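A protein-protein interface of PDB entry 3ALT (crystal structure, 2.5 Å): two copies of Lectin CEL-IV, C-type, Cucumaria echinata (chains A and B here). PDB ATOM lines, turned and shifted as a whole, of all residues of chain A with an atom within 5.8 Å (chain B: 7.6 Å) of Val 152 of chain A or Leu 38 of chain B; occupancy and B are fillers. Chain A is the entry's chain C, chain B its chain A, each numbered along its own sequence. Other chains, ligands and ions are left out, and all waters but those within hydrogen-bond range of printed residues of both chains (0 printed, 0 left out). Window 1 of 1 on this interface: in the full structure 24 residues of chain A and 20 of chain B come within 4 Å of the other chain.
Leu 38 of chain B touches three residues of chain A.
Of the printed residues of chain A, Ser 40 of chain B touches Cys 151 (3.5 Å).
Printed residues of chain A within 4 Å of Tyr 154 of chain B: Leu 38 and Pro 150.
The nearest residue of chain A that does not touch Leu 38 of chain B is Tyr 154 of chain A (4.2 Å).
The nearest printed residue of chain A that does not touch Phe 36 of chain B is Tyr 154 of chain A (6.4 Å).
O of Gly 37 of chain B sits at hydrogen-bond distance from N of Thr 155 of chain A, at 2.8 Å.
The backbone carbonyl oxygen (O) of His 153 of chain A lies within hydrogen-bond range of the backbone NH (N) of Ala 39 of chain B (3.1 Å).
SG of Cys 41 of chain B is disulfide-bonded to SG of Cys 151 of chain A (2.0 Å).
The side-chain sulfur of Cys 41 of chain B sits at hydrogen-bond distance from the backbone NH of Val 152 of chain A (3.3 Å).
Printed residues of chain B that touch a printed residue of chain A: Gln 35, Phe 36, Gly 37, Leu 38, Ala 39, Ser 40, Cys 41, Leu 46, Leu 149, Pro 150, Val 152 and Tyr 154.
Hydrophobic or aromatic side chains of chain B that line the printed part of chain A: Phe 36, Leu 38, Leu 46, Leu 149, Val 152 and Tyr 154.
Among the printed residues, no Asp or Glu carboxylate lies within 4 Å of a Lys or Arg side-chain nitrogen of the other chain.
N of Gly 49 of chain B sits at hydrogen-bond distance from O of Phe 36 of chain B (2.7 Å).
The backbone carbonyl oxygen (O) of Ala 47 of chain B is in hydrogen-bond range of the backbone NH (N) of Leu 38 of chain B (3.2 Å).
OG of Ser 42 of chain B lies within hydrogen-bond range of OG of Ser 40 of chain B (3.0 Å).
The backbone NH (N) of Gly 43 of chain B sits at hydrogen-bond distance from the side-chain hydroxyl (OG) of Ser 40 of chain B (3.1 Å).
OG of Ser 40 of chain B sits at hydrogen-bond distance from N of Asp 44 of chain B, 3.1 Å away.
The backbone NH of Leu 38 of chain A sits at hydrogen-bond distance from the backbone carbonyl oxygen of Ala 47 of chain A (3.1 Å).
Leu 38 of chain A touches Val 152 of chain B, and with the chains exchanged Val 152 of chain A touches Leu 38 of chain B.
Leu 38 of chain A touches Tyr 154 of chain B, but with the chains exchanged Tyr 154 of chain A does not touch Leu 38 of chain B (4.2 Å).
Leu 46 of chain A touches Val 152 of chain B, and with the chains exchanged Val 152 of chain A touches Leu 46 of chain B.
Pro 150 of chain A touches Tyr 154 of chain B, and with the chains exchanged Tyr 154 of chain A touches Pro 150 of chain B.
7 positions are printed for both chains.
Among the printed residues, pairs that only touch across the chains: Leu 38 of chain A with Val 152 of chain B (3.5 Å), Leu 38 of chain A with Tyr 154 of chain B (3.8 Å), Leu 46 of chain A with Leu 46 of chain B (3.5 Å), Leu 46 of chain A with Val 152 of chain B (3.3 Å), Pro 150 of chain A with Tyr 154 of chain B (3.9 Å), Cys 151 of chain A with Ser 40 of chain B (3.5 Å), Val 152 of chain A with Leu 38 of chain B (3.7 Å), Val 152 of chain A with Ala 39 of chain B (3.3 Å), Val 152 of chain A with Leu 46 of chain B (3.9 Å), His 153 of chain A with Leu 38 of chain B (3.4 Å), Tyr 154 of chain A with Gly 37 of chain B (3.3 Å), Tyr 154 of chain A with Leu 149 of chain B (3.6 Å), Tyr 154 of chain A with Pro 150 of chain B (3.8 Å), Thr 155 of chain A with Gln 35 of chain B (3.99 Å), Thr 155 of chain A with Phe 36 of chain B (3.2 Å) and Thr 155 of chain A with Leu 38 of chain B (3.5 Å).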
ATOM      1  N   GLY A  14     -34.919  17.216 -12.513  1.00  0.00           N
ATOM      2  CA  GLY A  14     -34.151  16.184 -13.203  1.00  0.00           C
ATOM      3  C   GLY A  14     -32.700  16.525 -13.495  1.00  0.00           C
ATOM      4  O   GLY A  14     -31.990  15.693 -14.053  1.00  0.00           O
ATOM      5  N   LEU A  38     -20.506  11.117 -16.778  1.00  0.00           N
ATOM      6  CA  LEU A  38     -21.429  10.003 -16.639  1.00  0.00           C
ATOM      7  C   LEU A  38     -20.756   8.752 -17.230  1.00  0.00           C
ATOM      8  O   LEU A  38     -20.051   8.851 -18.231  1.00  0.00           O
ATOM      9  CB  LEU A  38     -22.707  10.353 -17.390  1.00  0.00           C
ATOM     10  CG  LEU A  38     -24.026   9.625 -17.138  1.00  0.00           C
ATOM     11  CD1 LEU A  38     -24.076   8.408 -18.003  1.00  0.00           C
ATOM     12  CD2 LEU A  38     -24.227   9.219 -15.685  1.00  0.00           C
ATOM     13  N   LEU A  46     -19.622   8.019 -20.791  1.00  0.00           N
ATOM     14  CA  LEU A  46     -20.699   8.260 -21.760  1.00  0.00           C
ATOM     15  C   LEU A  46     -20.951   9.725 -22.082  1.00  0.00           C
ATOM     16  O   LEU A  46     -21.320  10.066 -23.205  1.00  0.00           O
ATOM     17  CB  LEU A  46     -22.006   7.628 -21.307  1.00  0.00           C
ATOM     18  CG  LEU A  46     -22.069   6.105 -21.199  1.00  0.00           C
ATOM     19  CD1 LEU A  46     -23.311   5.715 -20.438  1.00  0.00           C
ATOM     20  CD2 LEU A  46     -22.049   5.452 -22.563  1.00  0.00           C
ATOM     21  N   ALA A  47     -20.771  10.602 -21.104  1.00  0.00           N
ATOM     22  CA  ALA A  47     -20.972  12.043 -21.346  1.00  0.00           C
ATOM     23  C   ALA A  47     -20.128  12.837 -20.372  1.00  0.00           C
ATOM     24  O   ALA A  47     -19.431  12.265 -19.505  1.00  0.00           O
ATOM     25  CB  ALA A  47     -22.450  12.450 -21.245  1.00  0.00           C
ATOM     26  N   PRO A 150     -24.130  15.675 -16.454  1.00  0.00           N
ATOM     27  CA  PRO A 150     -24.764  15.273 -17.698  1.00  0.00           C
ATOM     28  C   PRO A 150     -26.246  14.992 -17.456  1.00  0.00           C
ATOM     29  O   PRO A 150     -26.586  14.128 -16.654  1.00  0.00           O
ATOM     30  CB  PRO A 150     -24.021  13.987 -18.085  1.00  0.00           C
ATOM     31  CG  PRO A 150     -22.791  13.908 -17.219  1.00  0.00           C
ATOM     32  CD  PRO A 150     -23.061  14.753 -16.019  1.00  0.00           C
ATOM     33  N   CYS A 151     -27.102  15.777 -18.102  1.00  0.00           N
ATOM     34  CA  CYS A 151     -28.549  15.643 -18.045  1.00  0.00           C
ATOM     35  C   CYS A 151     -29.004  14.447 -18.881  1.00  0.00           C
ATOM     36  O   CYS A 151     -28.706  14.387 -20.072  1.00  0.00           O
ATOM     37  CB  CYS A 151     -29.137  16.913 -18.634  1.00  0.00           C
ATOM     38  SG  CYS A 151     -30.932  17.011 -18.580  1.00  0.00           S
ATOM     39  N   VAL A 152     -29.740  13.507 -18.291  1.00  0.00           N
ATOM     40  CA  VAL A 152     -30.114  12.274 -19.032  1.00  0.00           C
ATOM     41  C   VAL A 152     -31.487  11.697 -18.657  1.00  0.00           C
ATOM     42  O   VAL A 152     -31.918  11.789 -17.483  1.00  0.00           O
ATOM     43  CB  VAL A 152     -29.099  11.119 -18.835  1.00  0.00           C
ATOM     44  CG1 VAL A 152     -27.826  11.380 -19.582  1.00  0.00           C
ATOM     45  CG2 VAL A 152     -28.864  10.803 -17.344  1.00  0.00           C
ATOM     46  N   HIS A 153     -32.164  11.073 -19.626  1.00  0.00           N
ATOM     47  CA  HIS A 153     -33.365  10.351 -19.251  1.00  0.00           C
ATOM     48  C   HIS A 153     -33.465   8.995 -19.921  1.00  0.00           C
ATOM     49  O   HIS A 153     -32.811   8.747 -20.919  1.00  0.00           O
ATOM     50  CB  HIS A 153     -34.605  11.221 -19.507  1.00  0.00           C
ATOM     51  CG  HIS A 153     -34.826  11.498 -20.949  1.00  0.00           C
ATOM     52  ND1 HIS A 153     -34.344  12.626 -21.567  1.00  0.00           N
ATOM     53  CD2 HIS A 153     -35.406  10.753 -21.921  1.00  0.00           C
ATOM     54  CE1 HIS A 153     -34.638  12.586 -22.856  1.00  0.00           C
ATOM     55  NE2 HIS A 153     -35.282  11.457 -23.098  1.00  0.00           N
ATOM     56  N   TYR A 154     -34.280   8.116 -19.347  1.00  0.00           N
ATOM     57  CA  TYR A 154     -34.555   6.823 -19.939  1.00  0.00           C
ATOM     58  C   TYR A 154     -35.542   6.996 -21.113  1.00  0.00           C
ATOM     59  O   TYR A 154     -36.437   7.855 -21.070  1.00  0.00           O
ATOM     60  CB  TYR A 154     -35.079   5.858 -18.878  1.00  0.00           C
ATOM     61  CG  TYR A 154     -34.080   5.460 -17.810  1.00  0.00           C
ATOM     62  CD1 TYR A 154     -32.939   4.709 -18.123  1.00  0.00           C
ATOM     63  CD2 TYR A 154     -34.300   5.791 -16.475  1.00  0.00           C
ATOM     64  CE1 TYR A 154     -32.026   4.305 -17.121  1.00  0.00           C
ATOM     65  CE2 TYR A 154     -33.405   5.406 -15.470  1.00  0.00           C
ATOM     66  CZ  TYR A 154     -32.272   4.659 -15.806  1.00  0.00           C
ATOM     67  OH  TYR A 154     -31.387   4.270 -14.839  1.00  0.00           O
ATOM     68  N   THR A 155     -35.331   6.209 -22.173  1.00  0.00           N
ATOM     69  CA  THR A 155     -36.254   6.130 -23.312  1.00  0.00           C
ATOM     70  C   THR A 155     -37.045   4.839 -23.406  1.00  0.00           C
ATOM     71  O   THR A 155     -36.480   3.725 -23.374  1.00  0.00           O
ATOM     72  CB  THR A 155     -35.532   6.249 -24.655  1.00  0.00           C
ATOM     73  OG1 THR A 155     -34.202   5.734 -24.545  1.00  0.00           O
ATOM     74  CG2 THR A 155     -35.471   7.699 -25.126  1.00  0.00           C
ATOM     75  N   GLN B  35     -34.825  -1.682 -27.364  1.00  0.00           N
ATOM     76  CA  GLN B  35     -35.757  -0.582 -27.676  1.00  0.00           C
ATOM     77  C   GLN B  35     -35.792   0.425 -26.542  1.00  0.00           C
ATOM     78  O   GLN B  35     -36.376   1.494 -26.677  1.00  0.00           O
ATOM     79  CB  GLN B  35     -37.180  -1.102 -27.948  1.00  0.00           C
ATOM     80  CG  GLN B  35     -37.280  -2.149 -29.053  1.00  0.00           C
ATOM     81  CD  GLN B  35     -36.600  -1.708 -30.344  1.00  0.00           C
ATOM     82  OE1 GLN B  35     -37.112  -0.862 -31.072  1.00  0.00           O
ATOM     83  NE2 GLN B  35     -35.438  -2.290 -30.636  1.00  0.00           N
ATOM     84  N   PHE B  36     -35.200   0.073 -25.401  1.00  0.00           N
ATOM     85  CA  PHE B  36     -35.169   0.993 -24.269  1.00  0.00           C
ATOM     86  C   PHE B  36     -33.791   1.609 -24.174  1.00  0.00           C
ATOM     87  O   PHE B  36     -32.799   0.902 -24.284  1.00  0.00           O
ATOM     88  CB  PHE B  36     -35.587   0.289 -22.960  1.00  0.00           C
ATOM     89  CG  PHE B  36     -36.928  -0.386 -23.055  1.00  0.00           C
ATOM     90  CD1 PHE B  36     -38.118   0.368 -23.115  1.00  0.00           C
ATOM     91  CD2 PHE B  36     -37.015  -1.750 -23.174  1.00  0.00           C
ATOM     92  CE1 PHE B  36     -39.360  -0.249 -23.266  1.00  0.00           C
ATOM     93  CE2 PHE B  36     -38.275  -2.376 -23.346  1.00  0.00           C
ATOM     94  CZ  PHE B  36     -39.436  -1.610 -23.393  1.00  0.00           C
ATOM     95  N   GLY B  37     -33.713   2.924 -23.981  1.00  0.00           N
ATOM     96  CA  GLY B  37     -32.402   3.562 -24.016  1.00  0.00           C
ATOM     97  C   GLY B  37     -32.122   4.626 -22.985  1.00  0.00           C
ATOM     98  O   GLY B  37     -32.913   4.853 -22.087  1.00  0.00           O
ATOM     99  N   LEU B  38     -30.982   5.284 -23.177  1.00  0.00           N
ATOM    100  CA  LEU B  38     -30.545   6.414 -22.392  1.00  0.00           C
ATOM    101  C   LEU B  38     -30.153   7.521 -23.373  1.00  0.00           C
ATOM    102  O   LEU B  38     -29.484   7.260 -24.410  1.00  0.00           O
ATOM    103  CB  LEU B  38     -29.342   5.998 -21.548  1.00  0.00           C
ATOM    104  CG  LEU B  38     -28.911   6.785 -20.314  1.00  0.00           C
ATOM    105  CD1 LEU B  38     -27.949   7.843 -20.748  1.00  0.00           C
ATOM    106  CD2 LEU B  38     -30.048   7.405 -19.564  1.00  0.00           C
ATOM    107  N   ALA B  39     -30.541   8.755 -23.056  1.00  0.00           N
ATOM    108  CA  ALA B  39     -30.282   9.867 -23.965  1.00  0.00           C
ATOM    109  C   ALA B  39     -29.876  11.137 -23.248  1.00  0.00           C
ATOM    110  O   ALA B  39     -30.371  11.406 -22.165  1.00  0.00           O
ATOM    111  CB  ALA B  39     -31.523  10.119 -24.850  1.00  0.00           C
ATOM    112  N   SER B  40     -28.985  11.925 -23.836  1.00  0.00           N
ATOM    113  CA  SER B  40     -28.784  13.296 -23.354  1.00  0.00           C
ATOM    114  C   SER B  40     -30.107  14.089 -23.501  1.00  0.00           C
ATOM    115  O   SER B  40     -30.970  13.780 -24.340  1.00  0.00           O
ATOM    116  CB  SER B  40     -27.663  13.994 -24.126  1.00  0.00           C
ATOM    117  OG  SER B  40     -28.144  14.510 -25.361  1.00  0.00           O
ATOM    118  N   CYS B  41     -30.276  15.119 -22.690  1.00  0.00           N
ATOM    119  CA  CYS B  41     -31.479  15.945 -22.793  1.00  0.00           C
ATOM    120  C   CYS B  41     -31.507  16.749 -24.098  1.00  0.00           C
ATOM    121  O   CYS B  41     -32.595  17.180 -24.554  1.00  0.00           O
ATOM    122  CB  CYS B  41     -31.604  16.824 -21.547  1.00  0.00           C
ATOM    123  SG  CYS B  41     -31.462  15.726 -20.040  1.00  0.00           S
ATOM    124  N   SER B  42     -30.311  16.901 -24.694  1.00  0.00           N
ATOM    125  CA  SER B  42     -30.113  17.590 -25.970  1.00  0.00           C
ATOM    126  C   SER B  42     -30.336  16.694 -27.193  1.00  0.00           C
ATOM    127  O   SER B  42     -30.212  17.172 -28.324  1.00  0.00           O
ATOM    128  CB  SER B  42     -28.737  18.286 -26.032  1.00  0.00           C
ATOM    129  OG  SER B  42     -27.644  17.406 -25.723  1.00  0.00           O
ATOM    130  N   GLY B  43     -30.670  15.416 -26.962  1.00  0.00           N
ATOM    131  CA  GLY B  43     -31.087  14.500 -28.043  1.00  0.00           C
ATOM    132  C   GLY B  43     -30.215  13.307 -28.456  1.00  0.00           C
ATOM    133  O   GLY B  43     -30.718  12.383 -29.086  1.00  0.00           O
ATOM    134  N   ASP B  44     -28.921  13.303 -28.126  1.00  0.00           N
ATOM    135  CA  ASP B  44     -28.052  12.212 -28.563  1.00  0.00           C
ATOM    136  C   ASP B  44     -28.366  10.948 -27.773  1.00  0.00           C
ATOM    137  O   ASP B  44     -28.421  11.003 -26.555  1.00  0.00           O
ATOM    138  CB  ASP B  44     -26.568  12.582 -28.399  1.00  0.00           C
ATOM    139  CG  ASP B  44     -26.198  13.920 -29.068  1.00  0.00           C
ATOM    140  OD1 ASP B  44     -26.983  14.440 -29.884  1.00  0.00           O
ATOM    141  OD2 ASP B  44     -25.114  14.471 -28.775  1.00  0.00           O
ATOM    142  N   GLU B  45     -28.579   9.826 -28.458  1.00  0.00           N
ATOM    143  CA  GLU B  45     -28.735   8.510 -27.801  1.00  0.00           C
ATOM    144  C   GLU B  45     -27.377   7.969 -27.263  1.00  0.00           C
ATOM    145  O   GLU B  45     -26.437   7.751 -28.036  1.00  0.00           O
ATOM    146  CB  GLU B  45     -29.414   7.498 -28.766  1.00  0.00           C
ATOM    147  CG  GLU B  45     -29.061   5.987 -28.514  1.00  0.00           C
ATOM    148  CD  GLU B  45     -30.160   5.143 -27.795  1.00  0.00           C
ATOM    149  OE1 GLU B  45     -30.104   3.881 -27.876  1.00  0.00           O
ATOM    150  OE2 GLU B  45     -31.063   5.725 -27.149  1.00  0.00           O
ATOM    151  N   LEU B  46     -27.278   7.756 -25.955  1.00  0.00           N
ATOM    152  CA  LEU B  46     -25.990   7.376 -25.359  1.00  0.00           C
ATOM    153  C   LEU B  46     -25.737   5.887 -25.100  1.00  0.00           C
ATOM    154  O   LEU B  46     -24.577   5.446 -25.137  1.00  0.00           O
ATOM    155  CB  LEU B  46     -25.780   8.099 -24.044  1.00  0.00           C
ATOM    156  CG  LEU B  46     -25.727   9.605 -24.129  1.00  0.00           C
ATOM    157  CD1 LEU B  46     -25.922  10.152 -22.721  1.00  0.00           C
ATOM    158  CD2 LEU B  46     -24.416  10.081 -24.822  1.00  0.00           C
ATOM    159  N   ALA B  47     -26.806   5.133 -24.804  1.00  0.00           N
ATOM    160  CA  ALA B  47     -26.694   3.702 -24.581  1.00  0.00           C
ATOM    161  C   ALA B  47     -28.016   2.986 -24.893  1.00  0.00           C
ATOM    162  O   ALA B  47     -29.045   3.620 -25.152  1.00  0.00           O
ATOM    163  CB  ALA B  47     -26.247   3.428 -23.149  1.00  0.00           C
ATOM    164  N   THR B  48     -27.978   1.653 -24.839  1.00  0.00           N
ATOM    165  CA  THR B  48     -29.150   0.811 -25.097  1.00  0.00           C
ATOM    166  C   THR B  48     -29.369  -0.140 -23.923  1.00  0.00           C
ATOM    167  O   THR B  48     -28.401  -0.503 -23.230  1.00  0.00           O
ATOM    168  CB  THR B  48     -28.892  -0.048 -26.312  1.00  0.00           C
ATOM    169  OG1 THR B  48     -28.343   0.782 -27.332  1.00  0.00           O
ATOM    170  CG2 THR B  48     -30.159  -0.661 -26.843  1.00  0.00           C
ATOM    171  N   GLY B  49     -30.628  -0.525 -23.689  1.00  0.00           N
ATOM    172  CA  GLY B  49     -30.934  -1.704 -22.859  1.00  0.00           C
ATOM    173  C   GLY B  49     -30.489  -3.098 -23.373  1.00  0.00           C
ATOM    174  O   GLY B  49     -29.799  -3.259 -24.408  1.00  0.00           O
ATOM    175  N   LEU B 149     -32.359  -1.530 -17.889  1.00  0.00           N
ATOM    176  CA  LEU B 149     -32.099  -0.238 -18.523  1.00  0.00           C
ATOM    177  C   LEU B 149     -30.633   0.056 -18.400  1.00  0.00           C
ATOM    178  O   LEU B 149     -29.977  -0.487 -17.501  1.00  0.00           O
ATOM    179  CB  LEU B 149     -32.887   0.866 -17.844  1.00  0.00           C
ATOM    180  CG  LEU B 149     -34.386   0.822 -18.101  1.00  0.00           C
ATOM    181  CD1 LEU B 149     -35.045   1.834 -17.237  1.00  0.00           C
ATOM    182  CD2 LEU B 149     -34.693   1.095 -19.522  1.00  0.00           C
ATOM    183  N   PRO B 150     -30.105   0.914 -19.285  1.00  0.00           N
ATOM    184  CA  PRO B 150     -28.667   1.130 -19.306  1.00  0.00           C
ATOM    185  C   PRO B 150     -28.187   1.471 -17.907  1.00  0.00           C
ATOM    186  O   PRO B 150     -28.694   2.422 -17.300  1.00  0.00           O
ATOM    187  CB  PRO B 150     -28.494   2.344 -20.221  1.00  0.00           C
ATOM    188  CG  PRO B 150     -29.782   2.467 -20.993  1.00  0.00           C
ATOM    189  CD  PRO B 150     -30.841   1.870 -20.127  1.00  0.00           C
ATOM    190  N   CYS B 151     -27.243   0.674 -17.396  1.00  0.00           N
ATOM    191  CA  CYS B 151     -26.656   0.870 -16.072  1.00  0.00           C
ATOM    192  C   CYS B 151     -25.621   1.966 -16.145  1.00  0.00           C
ATOM    193  O   CYS B 151     -24.777   1.961 -17.033  1.00  0.00           O
ATOM    194  CB  CYS B 151     -25.950  -0.408 -15.646  1.00  0.00           C
ATOM    195  SG  CYS B 151     -25.304  -0.411 -13.926  1.00  0.00           S
ATOM    196  N   VAL B 152     -25.596   2.873 -15.186  1.00  0.00           N
ATOM    197  CA  VAL B 152     -24.838   4.100 -15.397  1.00  0.00           C
ATOM    198  C   VAL B 152     -24.575   4.823 -14.066  1.00  0.00           C
ATOM    199  O   VAL B 152     -25.434   4.820 -13.169  1.00  0.00           O
ATOM    200  CB  VAL B 152     -25.691   4.910 -16.398  1.00  0.00           C
ATOM    201  CG1 VAL B 152     -26.500   6.044 -15.799  1.00  0.00           C
ATOM    202  CG2 VAL B 152     -25.052   5.073 -17.757  1.00  0.00           C
ATOM    203  N   TYR B 154     -22.336   8.401 -12.130  1.00  0.00           N
ATOM    204  CA  TYR B 154     -21.499   9.585 -12.241  1.00  0.00           C
ATOM    205  C   TYR B 154     -20.067   9.316 -11.785  1.00  0.00           C
ATOM    206  O   TYR B 154     -19.839   8.489 -10.894  1.00  0.00           O
ATOM    207  CB  TYR B 154     -22.072  10.702 -11.399  1.00  0.00           C
ATOM    208  CG  TYR B 154     -23.408  11.235 -11.859  1.00  0.00           C
ATOM    209  CD1 TYR B 154     -23.565  11.858 -13.104  1.00  0.00           C
ATOM    210  CD2 TYR B 154     -24.511  11.178 -11.027  1.00  0.00           C
ATOM    211  CE1 TYR B 154     -24.803  12.384 -13.514  1.00  0.00           C
ATOM    212  CE2 TYR B 154     -25.766  11.713 -11.427  1.00  0.00           C
ATOM    213  CZ  TYR B 154     -25.896  12.308 -12.663  1.00  0.00           C
ATOM    214  OH  TYR B 154     -27.129  12.809 -13.030  1.00  0.00           O
